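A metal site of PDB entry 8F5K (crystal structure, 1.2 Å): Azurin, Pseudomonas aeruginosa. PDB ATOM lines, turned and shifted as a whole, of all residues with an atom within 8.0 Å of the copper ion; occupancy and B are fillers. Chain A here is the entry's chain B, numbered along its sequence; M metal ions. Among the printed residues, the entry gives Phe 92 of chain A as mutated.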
ATOM      1  N   GLY A  29      24.828   1.030  12.126  1.00  0.00           N
ATOM      2  CA  GLY A  29      24.762   0.183  13.295  1.00  0.00           C
ATOM      3  C   GLY A  29      23.992  -1.084  12.928  1.00  0.00           C
ATOM      4  O   GLY A  29      22.896  -0.980  12.367  1.00  0.00           O
ATOM      5  N   ASN A  30      24.553  -2.233  13.203  1.00  0.00           N
ATOM      6  CA  ASN A  30      24.136  -3.453  12.545  1.00  0.00           C
ATOM      7  C   ASN A  30      23.693  -4.510  13.560  1.00  0.00           C
ATOM      8  O   ASN A  30      23.643  -4.284  14.774  1.00  0.00           O
ATOM      9  CB  ASN A  30      25.258  -3.959  11.640  1.00  0.00           C
ATOM     10  CG  ASN A  30      26.539  -4.202  12.398  1.00  0.00           C
ATOM     11  OD1 ASN A  30      26.514  -4.796  13.479  1.00  0.00           O
ATOM     12  ND2 ASN A  30      27.681  -3.758  11.857  1.00  0.00           N
ATOM     13  N   MET A  33      25.651  -5.720  16.755  1.00  0.00           N
ATOM     14  CA  MET A  33      25.805  -4.805  17.883  1.00  0.00           C
ATOM     15  C   MET A  33      27.111  -4.033  17.767  1.00  0.00           C
ATOM     16  O   MET A  33      27.858  -3.867  18.740  1.00  0.00           O
ATOM     17  CB  MET A  33      25.686  -5.537  19.227  1.00  0.00           C
ATOM     18  CG  MET A  33      25.330  -4.673  20.404  1.00  0.00           C
ATOM     19  SD  MET A  33      25.374  -5.485  21.995  1.00  0.00           S
ATOM     20  CE  MET A  33      27.134  -5.702  22.196  1.00  0.00           C
ATOM     21  N   GLN A  34      27.396  -3.570  16.546  1.00  0.00           N
ATOM     22  CA  GLN A  34      28.580  -2.793  16.243  1.00  0.00           C
ATOM     23  C   GLN A  34      28.174  -1.649  15.321  1.00  0.00           C
ATOM     24  O   GLN A  34      27.239  -1.779  14.537  1.00  0.00           O
ATOM     25  CB  GLN A  34      29.643  -3.656  15.559  1.00  0.00           C
ATOM     26  CG  GLN A  34      30.277  -4.653  16.488  1.00  0.00           C
ATOM     27  CD  GLN A  34      31.262  -5.525  15.769  1.00  0.00           C
ATOM     28  OE1 GLN A  34      30.939  -6.138  14.767  1.00  0.00           O
ATOM     29  NE2 GLN A  34      32.477  -5.582  16.264  1.00  0.00           N
ATOM     30  N   PHE A  35      28.871  -0.533  15.432  1.00  0.00           N
ATOM     31  CA  PHE A  35      28.926   0.406  14.319  1.00  0.00           C
ATOM     32  C   PHE A  35      29.949  -0.083  13.310  1.00  0.00           C
ATOM     33  O   PHE A  35      30.833  -0.915  13.622  1.00  0.00           O
ATOM     34  CB  PHE A  35      29.399   1.780  14.791  1.00  0.00           C
ATOM     35  CG  PHE A  35      28.448   2.507  15.709  1.00  0.00           C
ATOM     36  CD1 PHE A  35      27.180   2.899  15.291  1.00  0.00           C
ATOM     37  CD2 PHE A  35      28.830   2.827  16.980  1.00  0.00           C
ATOM     38  CE1 PHE A  35      26.346   3.593  16.134  1.00  0.00           C
ATOM     39  CE2 PHE A  35      27.996   3.517  17.814  1.00  0.00           C
ATOM     40  CZ  PHE A  35      26.749   3.908  17.398  1.00  0.00           C
ATOM     41  N   LEU A  53      23.194   8.060  10.134  1.00  0.00           N
ATOM     42  CA  LEU A  53      23.151   6.736  10.728  1.00  0.00           C
ATOM     43  C   LEU A  53      22.094   5.904  10.021  1.00  0.00           C
ATOM     44  O   LEU A  53      21.001   6.387   9.718  1.00  0.00           O
ATOM     45  CB  LEU A  53      22.758   6.835  12.204  1.00  0.00           C
ATOM     46  CG  LEU A  53      22.747   5.514  12.987  1.00  0.00           C
ATOM     47  CD1 LEU A  53      24.102   4.889  13.121  1.00  0.00           C
ATOM     48  CD2 LEU A  53      22.047   5.730  14.364  1.00  0.00           C
ATOM     49  N   HIS A  55      20.547   1.560   9.806  1.00  0.00           N
ATOM     50  CA  HIS A  55      20.510   0.242  10.442  1.00  0.00           C
ATOM     51  C   HIS A  55      20.275  -0.797   9.365  1.00  0.00           C
ATOM     52  O   HIS A  55      19.110  -1.083   8.997  1.00  0.00           O
ATOM     53  CB  HIS A  55      19.418   0.207  11.496  1.00  0.00           C
ATOM     54  CG  HIS A  55      19.509  -0.950  12.443  1.00  0.00           C
ATOM     55  ND1 HIS A  55      19.778  -2.239  12.045  1.00  0.00           N
ATOM     56  CD2 HIS A  55      19.335  -0.989  13.778  1.00  0.00           C
ATOM     57  CE1 HIS A  55      19.776  -3.021  13.102  1.00  0.00           C
ATOM     58  NE2 HIS A  55      19.494  -2.290  14.169  1.00  0.00           N
ATOM     59  N   LYS A  61      13.916  -2.408  16.695  1.00  0.00           N
ATOM     60  CA  LYS A  61      14.479  -1.403  17.594  1.00  0.00           C
ATOM     61  C   LYS A  61      14.505  -1.863  19.035  1.00  0.00           C
ATOM     62  O   LYS A  61      15.397  -1.451  19.776  1.00  0.00           O
ATOM     63  CB  LYS A  61      13.680  -0.102  17.462  1.00  0.00           C
ATOM     64  CG  LYS A  61      14.284   1.073  18.231  1.00  0.00           C
ATOM     65  CD  LYS A  61      13.683   2.394  17.841  1.00  0.00           C
ATOM     66  CE  LYS A  61      12.285   2.507  18.397  1.00  0.00           C
ATOM     67  NZ  LYS A  61      11.628   3.741  17.922  1.00  0.00           N
ATOM     68  N   VAL A  63      15.009  -4.937  20.154  1.00  0.00           N
ATOM     69  CA  VAL A  63      16.017  -5.967  20.345  1.00  0.00           C
ATOM     70  C   VAL A  63      17.409  -5.446  20.053  1.00  0.00           C
ATOM     71  O   VAL A  63      18.370  -5.841  20.723  1.00  0.00           O
ATOM     72  CB  VAL A  63      15.697  -7.180  19.427  1.00  0.00           C
ATOM     73  CG1 VAL A  63      16.875  -8.134  19.355  1.00  0.00           C
ATOM     74  CG2 VAL A  63      14.432  -7.888  19.869  1.00  0.00           C
ATOM     75  N   MET A  64      17.559  -4.610  19.049  1.00  0.00           N
ATOM     76  CA  MET A  64      18.858  -4.192  18.532  1.00  0.00           C
ATOM     77  C   MET A  64      18.781  -2.731  18.097  1.00  0.00           C
ATOM     78  O   MET A  64      19.278  -2.351  17.029  1.00  0.00           O
ATOM     79  CB  MET A  64      19.291  -5.096  17.378  1.00  0.00           C
ATOM     80  CG  MET A  64      20.714  -4.971  16.893  1.00  0.00           C
ATOM     81  SD  MET A  64      21.976  -5.182  18.164  1.00  0.00           S
ATOM     82  CE  MET A  64      21.901  -6.940  18.468  1.00  0.00           C
ATOM     83  N   GLY A  65      18.177  -1.890  18.924  1.00  0.00           N
ATOM     84  CA  GLY A  65      18.067  -0.481  18.588  1.00  0.00           C
ATOM     85  C   GLY A  65      19.406   0.212  18.719  1.00  0.00           C
ATOM     86  O   GLY A  65      20.230  -0.118  19.581  1.00  0.00           O
ATOM     87  N   HIS A  66      19.639   1.190  17.856  1.00  0.00           N
ATOM     88  CA  HIS A  66      20.872   1.937  17.867  1.00  0.00           C
ATOM     89  C   HIS A  66      20.605   3.416  17.728  1.00  0.00           C
ATOM     90  O   HIS A  66      19.738   3.839  16.942  1.00  0.00           O
ATOM     91  CB  HIS A  66      21.829   1.538  16.746  1.00  0.00           C
ATOM     92  CG  HIS A  66      22.203   0.101  16.731  1.00  0.00           C
ATOM     93  ND1 HIS A  66      22.612  -0.581  17.851  1.00  0.00           N
ATOM     94  CD2 HIS A  66      22.304  -0.775  15.693  1.00  0.00           C
ATOM     95  CE1 HIS A  66      22.906  -1.829  17.525  1.00  0.00           C
ATOM     96  NE2 HIS A  66      22.726  -1.974  16.223  1.00  0.00           N
ATOM     97  N   ASN A  67      21.355   4.201  18.465  1.00  0.00           N
ATOM     98  CA  ASN A  67      21.487   5.626  18.239  1.00  0.00           C
ATOM     99  C   ASN A  67      22.958   5.928  18.063  1.00  0.00           C
ATOM    100  O   ASN A  67      23.816   5.059  18.214  1.00  0.00           O
ATOM    101  CB  ASN A  67      20.796   6.469  19.324  1.00  0.00           C
ATOM    102  CG  ASN A  67      21.248   6.149  20.701  1.00  0.00           C
ATOM    103  OD1 ASN A  67      22.273   5.508  20.905  1.00  0.00           O
ATOM    104  ND2 ASN A  67      20.478   6.588  21.676  1.00  0.00           N
ATOM    105  N   TRP A  68      23.247   7.156  17.674  1.00  0.00           N
ATOM    106  CA  TRP A  68      24.620   7.651  17.567  1.00  0.00           C
ATOM    107  C   TRP A  68      24.680   8.872  18.473  1.00  0.00           C
ATOM    108  O   TRP A  68      23.955   9.846  18.241  1.00  0.00           O
ATOM    109  CB  TRP A  68      24.980   7.987  16.124  1.00  0.00           C
ATOM    110  CG  TRP A  68      26.430   8.337  15.979  1.00  0.00           C
ATOM    111  CD1 TRP A  68      27.448   7.478  15.741  1.00  0.00           C
ATOM    112  CD2 TRP A  68      27.015   9.645  16.104  1.00  0.00           C
ATOM    113  NE1 TRP A  68      28.643   8.162  15.700  1.00  0.00           N
ATOM    114  CE2 TRP A  68      28.404   9.485  15.910  1.00  0.00           C
ATOM    115  CE3 TRP A  68      26.498  10.912  16.350  1.00  0.00           C
ATOM    116  CZ2 TRP A  68      29.285  10.568  15.984  1.00  0.00           C
ATOM    117  CZ3 TRP A  68      27.380  11.986  16.406  1.00  0.00           C
ATOM    118  CH2 TRP A  68      28.758  11.808  16.219  1.00  0.00           C
ATOM    119  N   PHE A  92      16.409   6.040  25.106  1.00  0.00           N
ATOM    120  CA  PHE A  92      17.523   5.754  26.004  1.00  0.00           C
ATOM    121  C   PHE A  92      18.464   6.939  26.124  1.00  0.00           C
ATOM    122  O   PHE A  92      19.686   6.774  26.205  1.00  0.00           O
ATOM    123  CB  PHE A  92      18.245   4.480  25.612  1.00  0.00           C
ATOM    124  CG  PHE A  92      17.428   3.238  25.834  1.00  0.00           C
ATOM    125  CD1 PHE A  92      16.994   2.896  27.099  1.00  0.00           C
ATOM    126  CD2 PHE A  92      17.082   2.423  24.768  1.00  0.00           C
ATOM    127  CE1 PHE A  92      16.252   1.745  27.320  1.00  0.00           C
ATOM    128  CE2 PHE A  92      16.323   1.287  24.969  1.00  0.00           C
ATOM    129  CZ  PHE A  92      15.937   0.924  26.247  1.00  0.00           C
ATOM    130  N   LEU A 106      16.949   6.967  18.185  1.00  0.00           N
ATOM    131  CA  LEU A 106      17.107   5.520  18.224  1.00  0.00           C
ATOM    132  C   LEU A 106      16.381   4.915  17.033  1.00  0.00           C
ATOM    133  O   LEU A 106      15.214   5.242  16.784  1.00  0.00           O
ATOM    134  CB  LEU A 106      16.548   4.979  19.536  1.00  0.00           C
ATOM    135  CG  LEU A 106      16.877   3.543  19.880  1.00  0.00           C
ATOM    136  CD1 LEU A 106      18.321   3.417  20.367  1.00  0.00           C
ATOM    137  CD2 LEU A 106      15.880   3.023  20.950  1.00  0.00           C
ATOM    138  N   ILE A 107      17.048   3.998  16.344  1.00  0.00           N
ATOM    139  CA  ILE A 107      16.481   3.359  15.158  1.00  0.00           C
ATOM    140  C   ILE A 107      16.653   1.856  15.223  1.00  0.00           C
ATOM    141  O   ILE A 107      17.584   1.336  15.827  1.00  0.00           O
ATOM    142  CB  ILE A 107      17.108   3.887  13.858  1.00  0.00           C
ATOM    143  CG1 ILE A 107      18.620   3.652  13.817  1.00  0.00           C
ATOM    144  CG2 ILE A 107      16.818   5.347  13.649  1.00  0.00           C
ATOM    145  CD1 ILE A 107      19.246   4.008  12.450  1.00  0.00           C
ATOM    146  N   PHE A 131      28.965   6.689  20.658  1.00  0.00           N
ATOM    147  CA  PHE A 131      28.477   5.428  21.201  1.00  0.00           C
ATOM    148  C   PHE A 131      26.973   5.337  21.005  1.00  0.00           C
ATOM    149  O   PHE A 131      26.322   6.314  20.646  1.00  0.00           O
ATOM    150  CB  PHE A 131      28.858   5.313  22.679  1.00  0.00           C
ATOM    151  CG  PHE A 131      28.559   6.546  23.463  1.00  0.00           C
ATOM    152  CD1 PHE A 131      29.430   7.608  23.513  1.00  0.00           C
ATOM    153  CD2 PHE A 131      27.347   6.710  24.099  1.00  0.00           C
ATOM    154  CE1 PHE A 131      29.125   8.759  24.213  1.00  0.00           C
ATOM    155  CE2 PHE A 131      27.060   7.842  24.808  1.00  0.00           C
ATOM    156  CZ  PHE A 131      27.958   8.875  24.873  1.00  0.00           C
ATOM    157  N   CYS A 132      26.461   4.140  21.220  1.00  0.00           N
ATOM    158  CA  CYS A 132      25.051   3.845  21.299  1.00  0.00           C
ATOM    159  C   CYS A 132      24.668   3.720  22.767  1.00  0.00           C
ATOM    160  O   CYS A 132      25.405   3.097  23.545  1.00  0.00           O
ATOM    161  CB  CYS A 132      24.770   2.551  20.553  1.00  0.00           C
ATOM    162  SG  CYS A 132      23.034   2.048  20.667  1.00  0.00           S
ATOM    163  N   THR A 133      23.539   4.311  23.171  1.00  0.00           N
ATOM    164  CA  THR A 133      23.085   4.211  24.557  1.00  0.00           C
ATOM    165  C   THR A 133      22.027   3.137  24.762  1.00  0.00           C
ATOM    166  O   THR A 133      21.488   3.022  25.872  1.00  0.00           O
ATOM    167  CB  THR A 133      22.546   5.543  25.068  1.00  0.00           C
ATOM    168  OG1 THR A 133      21.427   5.951  24.270  1.00  0.00           O
ATOM    169  CG2 THR A 133      23.656   6.615  25.044  1.00  0.00           C
ATOM    170  N   PHE A 134      21.686   2.346  23.751  1.00  0.00           N
ATOM    171  CA  PHE A 134      20.791   1.227  24.011  1.00  0.00           C
ATOM    172  C   PHE A 134      21.440   0.319  25.043  1.00  0.00           C
ATOM    173  O   PHE A 134      22.643   0.046  24.951  1.00  0.00           O
ATOM    174  CB  PHE A 134      20.502   0.478  22.710  1.00  0.00           C
ATOM    175  CG  PHE A 134      19.527  -0.655  22.849  1.00  0.00           C
ATOM    176  CD1 PHE A 134      19.905  -1.836  23.433  1.00  0.00           C
ATOM    177  CD2 PHE A 134      18.220  -0.524  22.403  1.00  0.00           C
ATOM    178  CE1 PHE A 134      19.019  -2.881  23.540  1.00  0.00           C
ATOM    179  CE2 PHE A 134      17.332  -1.587  22.517  1.00  0.00           C
ATOM    180  CZ  PHE A 134      17.733  -2.746  23.082  1.00  0.00           C
ATOM    181  N   PRO A 135      20.693  -0.142  26.051  1.00  0.00           N
ATOM    182  CA  PRO A 135      21.302  -0.908  27.148  1.00  0.00           C
ATOM    183  C   PRO A 135      22.262  -1.986  26.675  1.00  0.00           C
ATOM    184  O   PRO A 135      21.930  -2.849  25.851  1.00  0.00           O
ATOM    185  CB  PRO A 135      20.085  -1.482  27.874  1.00  0.00           C
ATOM    186  CG  PRO A 135      19.051  -0.402  27.669  1.00  0.00           C
ATOM    187  CD  PRO A 135      19.263   0.081  26.280  1.00  0.00           C
ATOM    188  N   GLY A 136      23.478  -1.930  27.228  1.00  0.00           N
ATOM    189  CA  GLY A 136      24.523  -2.888  26.971  1.00  0.00           C
ATOM    190  C   GLY A 136      25.333  -2.639  25.723  1.00  0.00           C
ATOM    191  O   GLY A 136      26.475  -3.107  25.648  1.00  0.00           O
ATOM    192  N   HIS A 137      24.792  -1.917  24.739  1.00  0.00           N
ATOM    193  CA  HIS A 137      25.437  -1.865  23.434  1.00  0.00           C
ATOM    194  C   HIS A 137      26.813  -1.232  23.464  1.00  0.00           C
ATOM    195  O   HIS A 137      27.661  -1.596  22.649  1.00  0.00           O
ATOM    196  CB  HIS A 137      24.522  -1.149  22.457  1.00  0.00           C
ATOM    197  CG  HIS A 137      23.411  -2.002  21.986  1.00  0.00           C
ATOM    198  ND1 HIS A 137      22.662  -1.699  20.857  1.00  0.00           N
ATOM    199  CD2 HIS A 137      22.924  -3.167  22.475  1.00  0.00           C
ATOM    200  CE1 HIS A 137      21.778  -2.660  20.684  1.00  0.00           C
ATOM    201  NE2 HIS A 137      21.931  -3.570  21.634  1.00  0.00           N
ATOM    202  N   SER A 138      27.029  -0.284  24.383  1.00  0.00           N
ATOM    203  CA  SER A 138      28.310   0.399  24.482  1.00  0.00           C
ATOM    204  C   SER A 138      29.450  -0.557  24.793  1.00  0.00           C
ATOM    205  O   SER A 138      30.607  -0.137  24.693  1.00  0.00           O
ATOM    206  CB  SER A 138      28.254   1.552  25.508  1.00  0.00           C
ATOM    207  OG  SER A 138      28.120   1.047  26.814  1.00  0.00           O
ATOM    208  N   MET A 141      29.762  -0.809  21.026  1.00  0.00           N
ATOM    209  CA  MET A 141      29.394   0.367  20.235  1.00  0.00           C
ATOM    210  C   MET A 141      29.922   1.626  20.906  1.00  0.00           C
ATOM    211  O   MET A 141      29.211   2.452  21.480  1.00  0.00           O
ATOM    212  CB  MET A 141      27.896   0.406  20.036  1.00  0.00           C
ATOM    213  CG  MET A 141      27.421  -0.873  19.334  1.00  0.00           C
ATOM    214  SD  MET A 141      25.662  -0.805  18.947  1.00  0.00           S
ATOM    215  CE  MET A 141      25.696   0.236  17.490  1.00  0.00           C
HETATM  216 CU    CU M   1      22.762   0.021  19.780  1.00  0.00          CU
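O of His 66 is in hydrogen-bond range of N of Ile 107 (2.8 Å). SG of Cys 132 sits close to N of Asn 67 (3.5 Å). N of Cys 132 lies within hydrogen-bond range of O of Met 141 (3.2 Å). O of Asn 30 lies within hydrogen-bond range of NE2 of His 66 (2.9 Å). The side-chain sulfur (SD) of Met 141 lies close to a ring nitrogen (ND1) of His 66 (3.2 Å). SD of Met 141 sits close to ND1 of His 137 (3.7 Å). The side-chain sulfur (SG) of Cys 132 lies close to the backbone NH (N) of Phe 134 (3.4 Å).
CB of Phe 134 touches the copper ion (3.7 Å). SD of Met 141 touches the copper ion, at 3.1 Å. The nearest printed residue that does not touch the copper ion is Asn 67 (4.6 Å).
ND1 of His 66 binds the copper ion (2.0 Å). A ring nitrogen (ND1) of His 137 is bound to the copper ion. SG of Cys 132 is bound to the copper ion (2.2 Å). O of Gly 65 is bound to the copper ion (2.5 Å). The copper ion has four donor atoms within binding distance.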
